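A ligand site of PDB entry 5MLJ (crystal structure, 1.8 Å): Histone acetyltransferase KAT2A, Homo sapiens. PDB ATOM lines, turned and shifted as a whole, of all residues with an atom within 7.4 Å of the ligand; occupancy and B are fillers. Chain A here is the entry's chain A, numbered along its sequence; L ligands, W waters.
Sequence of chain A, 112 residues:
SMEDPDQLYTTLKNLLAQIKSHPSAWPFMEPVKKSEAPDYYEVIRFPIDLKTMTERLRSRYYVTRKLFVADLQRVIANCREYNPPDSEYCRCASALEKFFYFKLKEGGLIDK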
ATOM      1  N   ALA A  25      27.369  -0.974 -24.238  1.00  0.00           N
ATOM      2  CA  ALA A  25      26.220  -0.953 -23.322  1.00  0.00           C
ATOM      3  C   ALA A  25      25.645  -2.352 -23.045  1.00  0.00           C
ATOM      4  O   ALA A  25      24.898  -2.523 -22.079  1.00  0.00           O
ATOM      5  CB  ALA A  25      25.118  -0.033 -23.849  1.00  0.00           C
ATOM      6  N   TRP A  26      25.991  -3.330 -23.876  1.00  0.00           N
ATOM      7  CA  TRP A  26      25.324  -4.648 -23.845  1.00  0.00           C
ATOM      8  C   TRP A  26      25.259  -5.348 -22.462  1.00  0.00           C
ATOM      9  O   TRP A  26      24.234  -5.942 -22.158  1.00  0.00           O
ATOM     10  CB  TRP A  26      25.869  -5.609 -24.928  1.00  0.00           C
ATOM     11  CG  TRP A  26      27.271  -6.105 -24.732  1.00  0.00           C
ATOM     12  CD1 TRP A  26      28.406  -5.580 -25.262  1.00  0.00           C
ATOM     13  CD2 TRP A  26      27.682  -7.240 -23.953  1.00  0.00           C
ATOM     14  NE1 TRP A  26      29.508  -6.304 -24.857  1.00  0.00           N
ATOM     15  CE2 TRP A  26      29.090  -7.328 -24.052  1.00  0.00           C
ATOM     16  CE3 TRP A  26      27.004  -8.185 -23.174  1.00  0.00           C
ATOM     17  CZ2 TRP A  26      29.823  -8.317 -23.402  1.00  0.00           C
ATOM     18  CZ3 TRP A  26      27.728  -9.169 -22.534  1.00  0.00           C
ATOM     19  CH2 TRP A  26      29.129  -9.230 -22.653  1.00  0.00           C
ATOM     20  N   PRO A  27      26.309  -5.251 -21.631  1.00  0.00           N
ATOM     21  CA  PRO A  27      26.186  -5.942 -20.335  1.00  0.00           C
ATOM     22  C   PRO A  27      25.188  -5.293 -19.374  1.00  0.00           C
ATOM     23  O   PRO A  27      24.736  -5.934 -18.420  1.00  0.00           O
ATOM     24  CB  PRO A  27      27.609  -5.855 -19.746  1.00  0.00           C
ATOM     25  CG  PRO A  27      28.491  -5.493 -20.891  1.00  0.00           C
ATOM     26  CD  PRO A  27      27.634  -4.626 -21.763  1.00  0.00           C
ATOM     27  N   PHE A  28      24.837  -4.030 -19.637  1.00  0.00           N
ATOM     28  CA  PHE A  28      24.105  -3.205 -18.682  1.00  0.00           C
ATOM     29  C   PHE A  28      22.684  -2.886 -19.136  1.00  0.00           C
ATOM     30  O   PHE A  28      22.015  -2.046 -18.535  1.00  0.00           O
ATOM     31  CB  PHE A  28      24.886  -1.913 -18.469  1.00  0.00           C
ATOM     32  CG  PHE A  28      26.359  -2.147 -18.259  1.00  0.00           C
ATOM     33  CD1 PHE A  28      26.815  -2.736 -17.087  1.00  0.00           C
ATOM     34  CD2 PHE A  28      27.285  -1.805 -19.237  1.00  0.00           C
ATOM     35  CE1 PHE A  28      28.163  -2.962 -16.891  1.00  0.00           C
ATOM     36  CE2 PHE A  28      28.632  -2.031 -19.040  1.00  0.00           C
ATOM     37  CZ  PHE A  28      29.072  -2.609 -17.867  1.00  0.00           C
ATOM     38  N   MET A  29      22.212  -3.547 -20.194  1.00  0.00           N
ATOM     39  CA  MET A  29      20.907  -3.224 -20.774  1.00  0.00           C
ATOM     40  C   MET A  29      19.744  -3.670 -19.913  1.00  0.00           C
ATOM     41  O   MET A  29      18.690  -3.016 -19.900  1.00  0.00           O
ATOM     42  CB  MET A  29      20.795  -3.832 -22.174  1.00  0.00           C
ATOM     43  CG  MET A  29      21.704  -3.175 -23.204  1.00  0.00           C
ATOM     44  SD  MET A  29      21.242  -1.481 -23.575  1.00  0.00           S
ATOM     45  CE  MET A  29      19.738  -1.723 -24.519  1.00  0.00           C
ATOM     46  N   GLU A  30      19.915  -4.786 -19.200  1.00  0.00           N
ATOM     47  CA  GLU A  30      18.890  -5.331 -18.335  1.00  0.00           C
ATOM     48  C   GLU A  30      19.483  -5.774 -16.992  1.00  0.00           C
ATOM     49  O   GLU A  30      20.694  -5.965 -16.889  1.00  0.00           O
ATOM     50  CB  GLU A  30      18.219  -6.524 -19.017  1.00  0.00           C
ATOM     51  CG  GLU A  30      17.488  -6.156 -20.291  1.00  0.00           C
ATOM     52  CD  GLU A  30      16.744  -7.323 -20.868  1.00  0.00           C
ATOM     53  OE1 GLU A  30      17.398  -8.363 -21.136  1.00  0.00           O
ATOM     54  OE2 GLU A  30      15.510  -7.216 -21.060  1.00  0.00           O
ATOM     55  N   PRO A  31      18.634  -5.925 -15.961  1.00  0.00           N
ATOM     56  CA  PRO A  31      19.165  -6.258 -14.636  1.00  0.00           C
ATOM     57  C   PRO A  31      19.949  -7.567 -14.597  1.00  0.00           C
ATOM     58  O   PRO A  31      19.630  -8.500 -15.331  1.00  0.00           O
ATOM     59  CB  PRO A  31      17.909  -6.384 -13.762  1.00  0.00           C
ATOM     60  CG  PRO A  31      16.836  -5.682 -14.489  1.00  0.00           C
ATOM     61  CD  PRO A  31      17.167  -5.792 -15.949  1.00  0.00           C
ATOM     62  N   VAL A  32      20.969  -7.615 -13.743  1.00  0.00           N
ATOM     63  CA  VAL A  32      21.749  -8.832 -13.534  1.00  0.00           C
ATOM     64  C   VAL A  32      20.815  -9.935 -13.040  1.00  0.00           C
ATOM     65  O   VAL A  32      19.945  -9.692 -12.202  1.00  0.00           O
ATOM     66  CB  VAL A  32      22.891  -8.606 -12.520  1.00  0.00           C
ATOM     67  CG1 VAL A  32      23.590  -9.907 -12.156  1.00  0.00           C
ATOM     68  CG2 VAL A  32      23.902  -7.601 -13.078  1.00  0.00           C
ATOM     69  N   LYS A  33      20.951 -11.135 -13.597  1.00  0.00           N
ATOM     70  CA  LYS A  33      20.117 -12.260 -13.208  1.00  0.00           C
ATOM     71  C   LYS A  33      20.809 -13.085 -12.137  1.00  0.00           C
ATOM     72  O   LYS A  33      22.029 -13.216 -12.144  1.00  0.00           O
ATOM     73  CB  LYS A  33      19.791 -13.127 -14.423  1.00  0.00           C
ATOM     74  CG  LYS A  33      18.910 -12.417 -15.441  1.00  0.00           C
ATOM     75  CD  LYS A  33      18.343 -13.361 -16.482  1.00  0.00           C
ATOM     76  CE  LYS A  33      19.394 -13.809 -17.488  1.00  0.00           C
ATOM     77  NZ  LYS A  33      18.760 -14.377 -18.719  1.00  0.00           N
ATOM     78  N   GLU A  36      23.154 -15.706 -13.305  1.00  0.00           N
ATOM     79  CA  GLU A  36      24.471 -15.205 -13.685  1.00  0.00           C
ATOM     80  C   GLU A  36      25.362 -14.979 -12.476  1.00  0.00           C
ATOM     81  O   GLU A  36      26.572 -15.235 -12.522  1.00  0.00           O
ATOM     82  CB  GLU A  36      24.323 -13.881 -14.451  1.00  0.00           C
ATOM     83  CG  GLU A  36      23.565 -14.019 -15.769  1.00  0.00           C
ATOM     84  CD  GLU A  36      23.170 -12.686 -16.381  1.00  0.00           C
ATOM     85  OE1 GLU A  36      22.986 -11.707 -15.629  1.00  0.00           O
ATOM     86  OE2 GLU A  36      23.035 -12.633 -17.616  1.00  0.00           O
ATOM     87  N   ALA A  37      24.770 -14.485 -11.396  1.00  0.00           N
ATOM     88  CA  ALA A  37      25.502 -14.099 -10.189  1.00  0.00           C
ATOM     89  C   ALA A  37      24.562 -14.256  -8.982  1.00  0.00           C
ATOM     90  O   ALA A  37      23.848 -13.316  -8.631  1.00  0.00           O
ATOM     91  CB  ALA A  37      25.991 -12.661 -10.311  1.00  0.00           C
ATOM     92  N   TYR A  40      24.403 -11.625  -6.165  1.00  0.00           N
ATOM     93  CA  TYR A  40      24.483 -10.228  -6.614  1.00  0.00           C
ATOM     94  C   TYR A  40      23.635  -9.277  -5.784  1.00  0.00           C
ATOM     95  O   TYR A  40      24.093  -8.189  -5.420  1.00  0.00           O
ATOM     96  CB  TYR A  40      24.085 -10.104  -8.085  1.00  0.00           C
ATOM     97  CG  TYR A  40      24.435  -8.754  -8.679  1.00  0.00           C
ATOM     98  CD1 TYR A  40      25.723  -8.499  -9.145  1.00  0.00           C
ATOM     99  CD2 TYR A  40      23.489  -7.735  -8.766  1.00  0.00           C
ATOM    100  CE1 TYR A  40      26.060  -7.269  -9.677  1.00  0.00           C
ATOM    101  CE2 TYR A  40      23.818  -6.500  -9.298  1.00  0.00           C
ATOM    102  CZ  TYR A  40      25.098  -6.275  -9.753  1.00  0.00           C
ATOM    103  OH  TYR A  40      25.435  -5.045 -10.285  1.00  0.00           O
ATOM    104  N   ILE A  44      25.374  -6.244  -3.959  1.00  0.00           N
ATOM    105  CA  ILE A  44      25.073  -4.933  -4.546  1.00  0.00           C
ATOM    106  C   ILE A  44      23.684  -4.486  -4.091  1.00  0.00           C
ATOM    107  O   ILE A  44      22.681  -5.045  -4.530  1.00  0.00           O
ATOM    108  CB  ILE A  44      25.156  -4.997  -6.093  1.00  0.00           C
ATOM    109  CG1 ILE A  44      26.577  -5.393  -6.540  1.00  0.00           C
ATOM    110  CG2 ILE A  44      24.735  -3.684  -6.723  1.00  0.00           C
ATOM    111  CD1 ILE A  44      27.665  -4.417  -6.141  1.00  0.00           C
ATOM    112  N   ILE A  48      21.298  -1.374 -10.618  1.00  0.00           N
ATOM    113  CA  ILE A  48      20.744  -0.467 -11.617  1.00  0.00           C
ATOM    114  C   ILE A  48      21.241  -0.902 -12.993  1.00  0.00           C
ATOM    115  O   ILE A  48      22.287  -1.521 -13.127  1.00  0.00           O
ATOM    116  CB  ILE A  48      21.097   0.996 -11.251  1.00  0.00           C
ATOM    117  CG1 ILE A  48      20.357   2.013 -12.141  1.00  0.00           C
ATOM    118  CG2 ILE A  48      22.600   1.241 -11.299  1.00  0.00           C
ATOM    119  CD1 ILE A  48      18.849   2.014 -11.975  1.00  0.00           C
ATOM    120  N   VAL A  75      25.704   2.371 -12.327  1.00  0.00           N
ATOM    121  CA  VAL A  75      25.835   1.229 -13.245  1.00  0.00           C
ATOM    122  C   VAL A  75      27.311   0.815 -13.314  1.00  0.00           C
ATOM    123  O   VAL A  75      27.650  -0.362 -13.182  1.00  0.00           O
ATOM    124  CB  VAL A  75      25.340   1.535 -14.682  1.00  0.00           C
ATOM    125  CG1 VAL A  75      25.710   0.418 -15.644  1.00  0.00           C
ATOM    126  CG2 VAL A  75      23.836   1.761 -14.699  1.00  0.00           C
ATOM    127  N   ASN A  78      28.814  -0.175  -9.583  1.00  0.00           N
ATOM    128  CA  ASN A  78      28.379  -1.529  -9.215  1.00  0.00           C
ATOM    129  C   ASN A  78      29.200  -2.588  -9.942  1.00  0.00           C
ATOM    130  O   ASN A  78      29.624  -3.574  -9.345  1.00  0.00           O
ATOM    131  CB  ASN A  78      26.886  -1.748  -9.519  1.00  0.00           C
ATOM    132  CG  ASN A  78      25.953  -1.056  -8.531  1.00  0.00           C
ATOM    133  OD1 ASN A  78      26.367  -0.559  -7.488  1.00  0.00           O
ATOM    134  ND2 ASN A  78      24.675  -1.045  -8.859  1.00  0.00           N
ATOM    135  N   CYS A  79      29.410  -2.378 -11.238  1.00  0.00           N
ATOM    136  CA  CYS A  79      30.191  -3.287 -12.054  1.00  0.00           C
ATOM    137  C   CYS A  79      31.620  -3.430 -11.513  1.00  0.00           C
ATOM    138  O   CYS A  79      32.144  -4.537 -11.421  1.00  0.00           O
ATOM    139  CB  CYS A  79      30.211  -2.821 -13.513  1.00  0.00           C
ATOM    140  SG  CYS A  79      31.090  -3.925 -14.643  1.00  0.00           S
ATOM    141  N   ARG A  80      32.231  -2.307 -11.148  1.00  0.00           N
ATOM    142  CA  ARG A  80      33.598  -2.305 -10.604  1.00  0.00           C
ATOM    143  C   ARG A  80      33.687  -2.876  -9.191  1.00  0.00           C
ATOM    144  O   ARG A  80      34.723  -3.405  -8.794  1.00  0.00           O
ATOM    145  CB  ARG A  80      34.192  -0.895 -10.652  1.00  0.00           C
ATOM    146  CG  ARG A  80      34.492  -0.439 -12.076  1.00  0.00           C
ATOM    147  CD  ARG A  80      34.993   0.993 -12.129  1.00  0.00           C
ATOM    148  NE  ARG A  80      35.357   1.340 -13.505  1.00  0.00           N
ATOM    149  CZ  ARG A  80      35.344   2.578 -14.027  1.00  0.00           C
ATOM    150  NH1 ARG A  80      34.996   3.635 -13.307  1.00  0.00           N
ATOM    151  NH2 ARG A  80      35.691   2.740 -15.291  1.00  0.00           N
ATOM    152  N   TYR A  82      31.567  -5.365  -8.005  1.00  0.00           N
ATOM    153  CA  TYR A  82      31.262  -6.797  -8.054  1.00  0.00           C
ATOM    154  C   TYR A  82      32.254  -7.636  -8.853  1.00  0.00           C
ATOM    155  O   TYR A  82      32.588  -8.751  -8.450  1.00  0.00           O
ATOM    156  CB  TYR A  82      29.851  -7.055  -8.592  1.00  0.00           C
ATOM    157  CG  TYR A  82      29.424  -8.479  -8.363  1.00  0.00           C
ATOM    158  CD1 TYR A  82      28.903  -8.875  -7.138  1.00  0.00           C
ATOM    159  CD2 TYR A  82      29.617  -9.462  -9.336  1.00  0.00           C
ATOM    160  CE1 TYR A  82      28.531 -10.192  -6.903  1.00  0.00           C
ATOM    161  CE2 TYR A  82      29.267 -10.781  -9.113  1.00  0.00           C
ATOM    162  CZ  TYR A  82      28.723 -11.139  -7.897  1.00  0.00           C
ATOM    163  OH  TYR A  82      28.365 -12.452  -7.653  1.00  0.00           O
ATOM    164  N   ASN A  83      32.693  -7.114  -9.994  1.00  0.00           N
ATOM    165  CA  ASN A  83      33.484  -7.904 -10.933  1.00  0.00           C
ATOM    166  C   ASN A  83      34.984  -7.718 -10.769  1.00  0.00           C
ATOM    167  O   ASN A  83      35.415  -6.710 -10.193  1.00  0.00           O
ATOM    168  CB  ASN A  83      33.064  -7.574 -12.365  1.00  0.00           C
ATOM    169  CG  ASN A  83      31.626  -7.934 -12.650  1.00  0.00           C
ATOM    170  OD1 ASN A  83      31.267  -9.117 -12.668  1.00  0.00           O
ATOM    171  ND2 ASN A  83      30.791  -6.933 -12.873  1.00  0.00           N
ATOM    172  N   TYR A  89      33.348  -7.391 -18.433  1.00  0.00           N
ATOM    173  CA  TYR A  89      32.342  -6.438 -17.934  1.00  0.00           C
ATOM    174  C   TYR A  89      32.980  -5.107 -17.543  1.00  0.00           C
ATOM    175  O   TYR A  89      32.473  -4.046 -17.895  1.00  0.00           O
ATOM    176  CB  TYR A  89      31.553  -7.011 -16.762  1.00  0.00           C
ATOM    177  CG  TYR A  89      30.659  -8.190 -17.101  1.00  0.00           C
ATOM    178  CD1 TYR A  89      30.071  -8.326 -18.358  1.00  0.00           C
ATOM    179  CD2 TYR A  89      30.384  -9.168 -16.144  1.00  0.00           C
ATOM    180  CE1 TYR A  89      29.252  -9.409 -18.661  1.00  0.00           C
ATOM    181  CE2 TYR A  89      29.566 -10.251 -16.437  1.00  0.00           C
ATOM    182  CZ  TYR A  89      29.008 -10.358 -17.697  1.00  0.00           C
ATOM    183  OH  TYR A  89      28.194 -11.432 -17.990  1.00  0.00           O
ATOM    184  N   CYS A  90      34.103  -5.167 -16.825  1.00  0.00           N
ATOM    185  CA  CYS A  90      34.798  -3.932 -16.436  1.00  0.00           C
ATOM    186  C   CYS A  90      35.370  -3.176 -17.648  1.00  0.00           C
ATOM    187  O   CYS A  90      35.352  -1.947 -17.669  1.00  0.00           O
ATOM    188  CB  CYS A  90      35.857  -4.196 -15.371  1.00  0.00           C
ATOM    189  SG  CYS A  90      35.138  -4.305 -13.707  1.00  0.00           S
HETATM  190  C1  LIG L   1      24.731 -11.723 -22.189  1.00  0.00           C
HETATM  191  C2  LIG L   1      24.892 -11.828 -23.559  1.00  0.00           C
HETATM  192  C3  LIG L   1      24.481 -10.802 -24.387  1.00  0.00           C
HETATM  193  C4  LIG L   1      23.910  -9.671 -23.835  1.00  0.00           C
HETATM  194  C5  LIG L   1      23.749  -9.566 -22.465  1.00  0.00           C
HETATM  195  C6  LIG L   1      20.978  -9.718 -17.939  1.00  0.00           C
HETATM  196  N1  LIG L   1      22.363 -10.050 -18.265  1.00  0.00           N
HETATM  197  C7  LIG L   1      23.286  -9.090 -17.656  1.00  0.00           C
HETATM  198  C8  LIG L   1      24.720  -9.498 -17.923  1.00  0.00           C
HETATM  199  C9  LIG L   1      24.959  -9.505 -19.439  1.00  0.00           C
HETATM  200  C10 LIG L   1      23.991 -10.475 -20.116  1.00  0.00           C
HETATM  201  C11 LIG L   1      22.551 -10.141 -19.727  1.00  0.00           C
HETATM  202  C12 LIG L   1      24.166 -10.583 -21.617  1.00  0.00           C
HETATM  203  N2  LIG L   1      25.629  -8.584 -17.222  1.00  0.00           N
HETATM  204  C13 LIG L   1      26.190  -8.824 -16.020  1.00  0.00           C
HETATM  205  C14 LIG L   1      26.094 -10.108 -15.411  1.00  0.00           C
HETATM  206  N3  LIG L   1      26.604 -10.424 -14.264  1.00  0.00           N
HETATM  207  N4  LIG L   1      27.271  -9.442 -13.591  1.00  0.00           N
HETATM  208  C15 LIG L   1      27.815  -9.845 -12.305  1.00  0.00           C
HETATM  209  C16 LIG L   1      27.462  -8.151 -14.035  1.00  0.00           C
HETATM  210  O1  LIG L   1      28.072  -7.334 -13.367  1.00  0.00           O
HETATM  211  C17 LIG L   1      26.868  -7.883 -15.326  1.00  0.00           C
HETATM  212 BR1  LIG L   1      27.104  -6.132 -15.958  1.00  0.00          BR
HETATM  213  O   HOH W   1      27.224 -12.334 -20.050  1.00  0.00           O
HETATM  214  O   HOH W   2      27.298  -4.895 -12.105  1.00  0.00           O
HETATM  215  O   HOH W   3      27.638 -13.357 -22.728  1.00  0.00           O
HETATM  216  O   HOH W   4      26.876 -13.154 -16.647  1.00  0.00           O
HETATM  217  O   HOH W   5      22.459  -6.576 -24.285  1.00  0.00           O
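Trp 26 touches the ligand (CE3 to C4, 3.5 Å).
Phe 28 touches the ligand.
O of Glu 30 touches C6 of the ligand (3.9 Å).
O of Pro 31 touches C6 of the ligand, at 3.2 Å.
Val 32 touches the ligand (CG1 to N3, 3.7 Å).
Ala 37 touches the ligand.
Tyr 82 touches the ligand.
Tyr 89 touches the ligand (OH to C14, 3.6 Å).
Hydrophobic or aromatic side chains that line the ligand: Trp 26, Pro 27, Phe 28, Val 32, Ala 37, Tyr 82 and Tyr 89.
Within 4 Å of the ligand: Trp 26, Pro 27, Phe 28, Glu 30, Pro 31, Val 32, Glu 36, Ala 37, Tyr 82, Asn 83 and Tyr 89.
The nearest printed residue that does not touch the ligand is Tyr 40 (4.02 Å).
The side-chain carboxylate (OE2) of Glu 36 lies within salt-bridge range of a nitrogen (N1) of the ligand, at 2.7 Å.
ND2 of Asn 83 is in hydrogen-bond range of O1 of the ligand, at 2.8 Å.
O of Pro 27 sits at hydrogen-bond distance from N2 of the ligand, at 3.0 Å.
Water W2 lies within hydrogen-bond range of the side-chain hydroxyl of Tyr 40 (2.6 Å), an oxygen (O1) of the ligand (2.9 Å) and the backbone NH of Cys 79 (3.4 Å).
The backbone NH (N) of Lys 33 sits at hydrogen-bond distance from the side-chain carboxylate (OE1) of Glu 36.
O of Cys 79 lies within hydrogen-bond range of ND2 of Asn 83, at 3.1 Å.
The backbone carbonyl oxygen of Tyr 89 lies within hydrogen-bond range of the side-chain sulfur of Cys 79.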
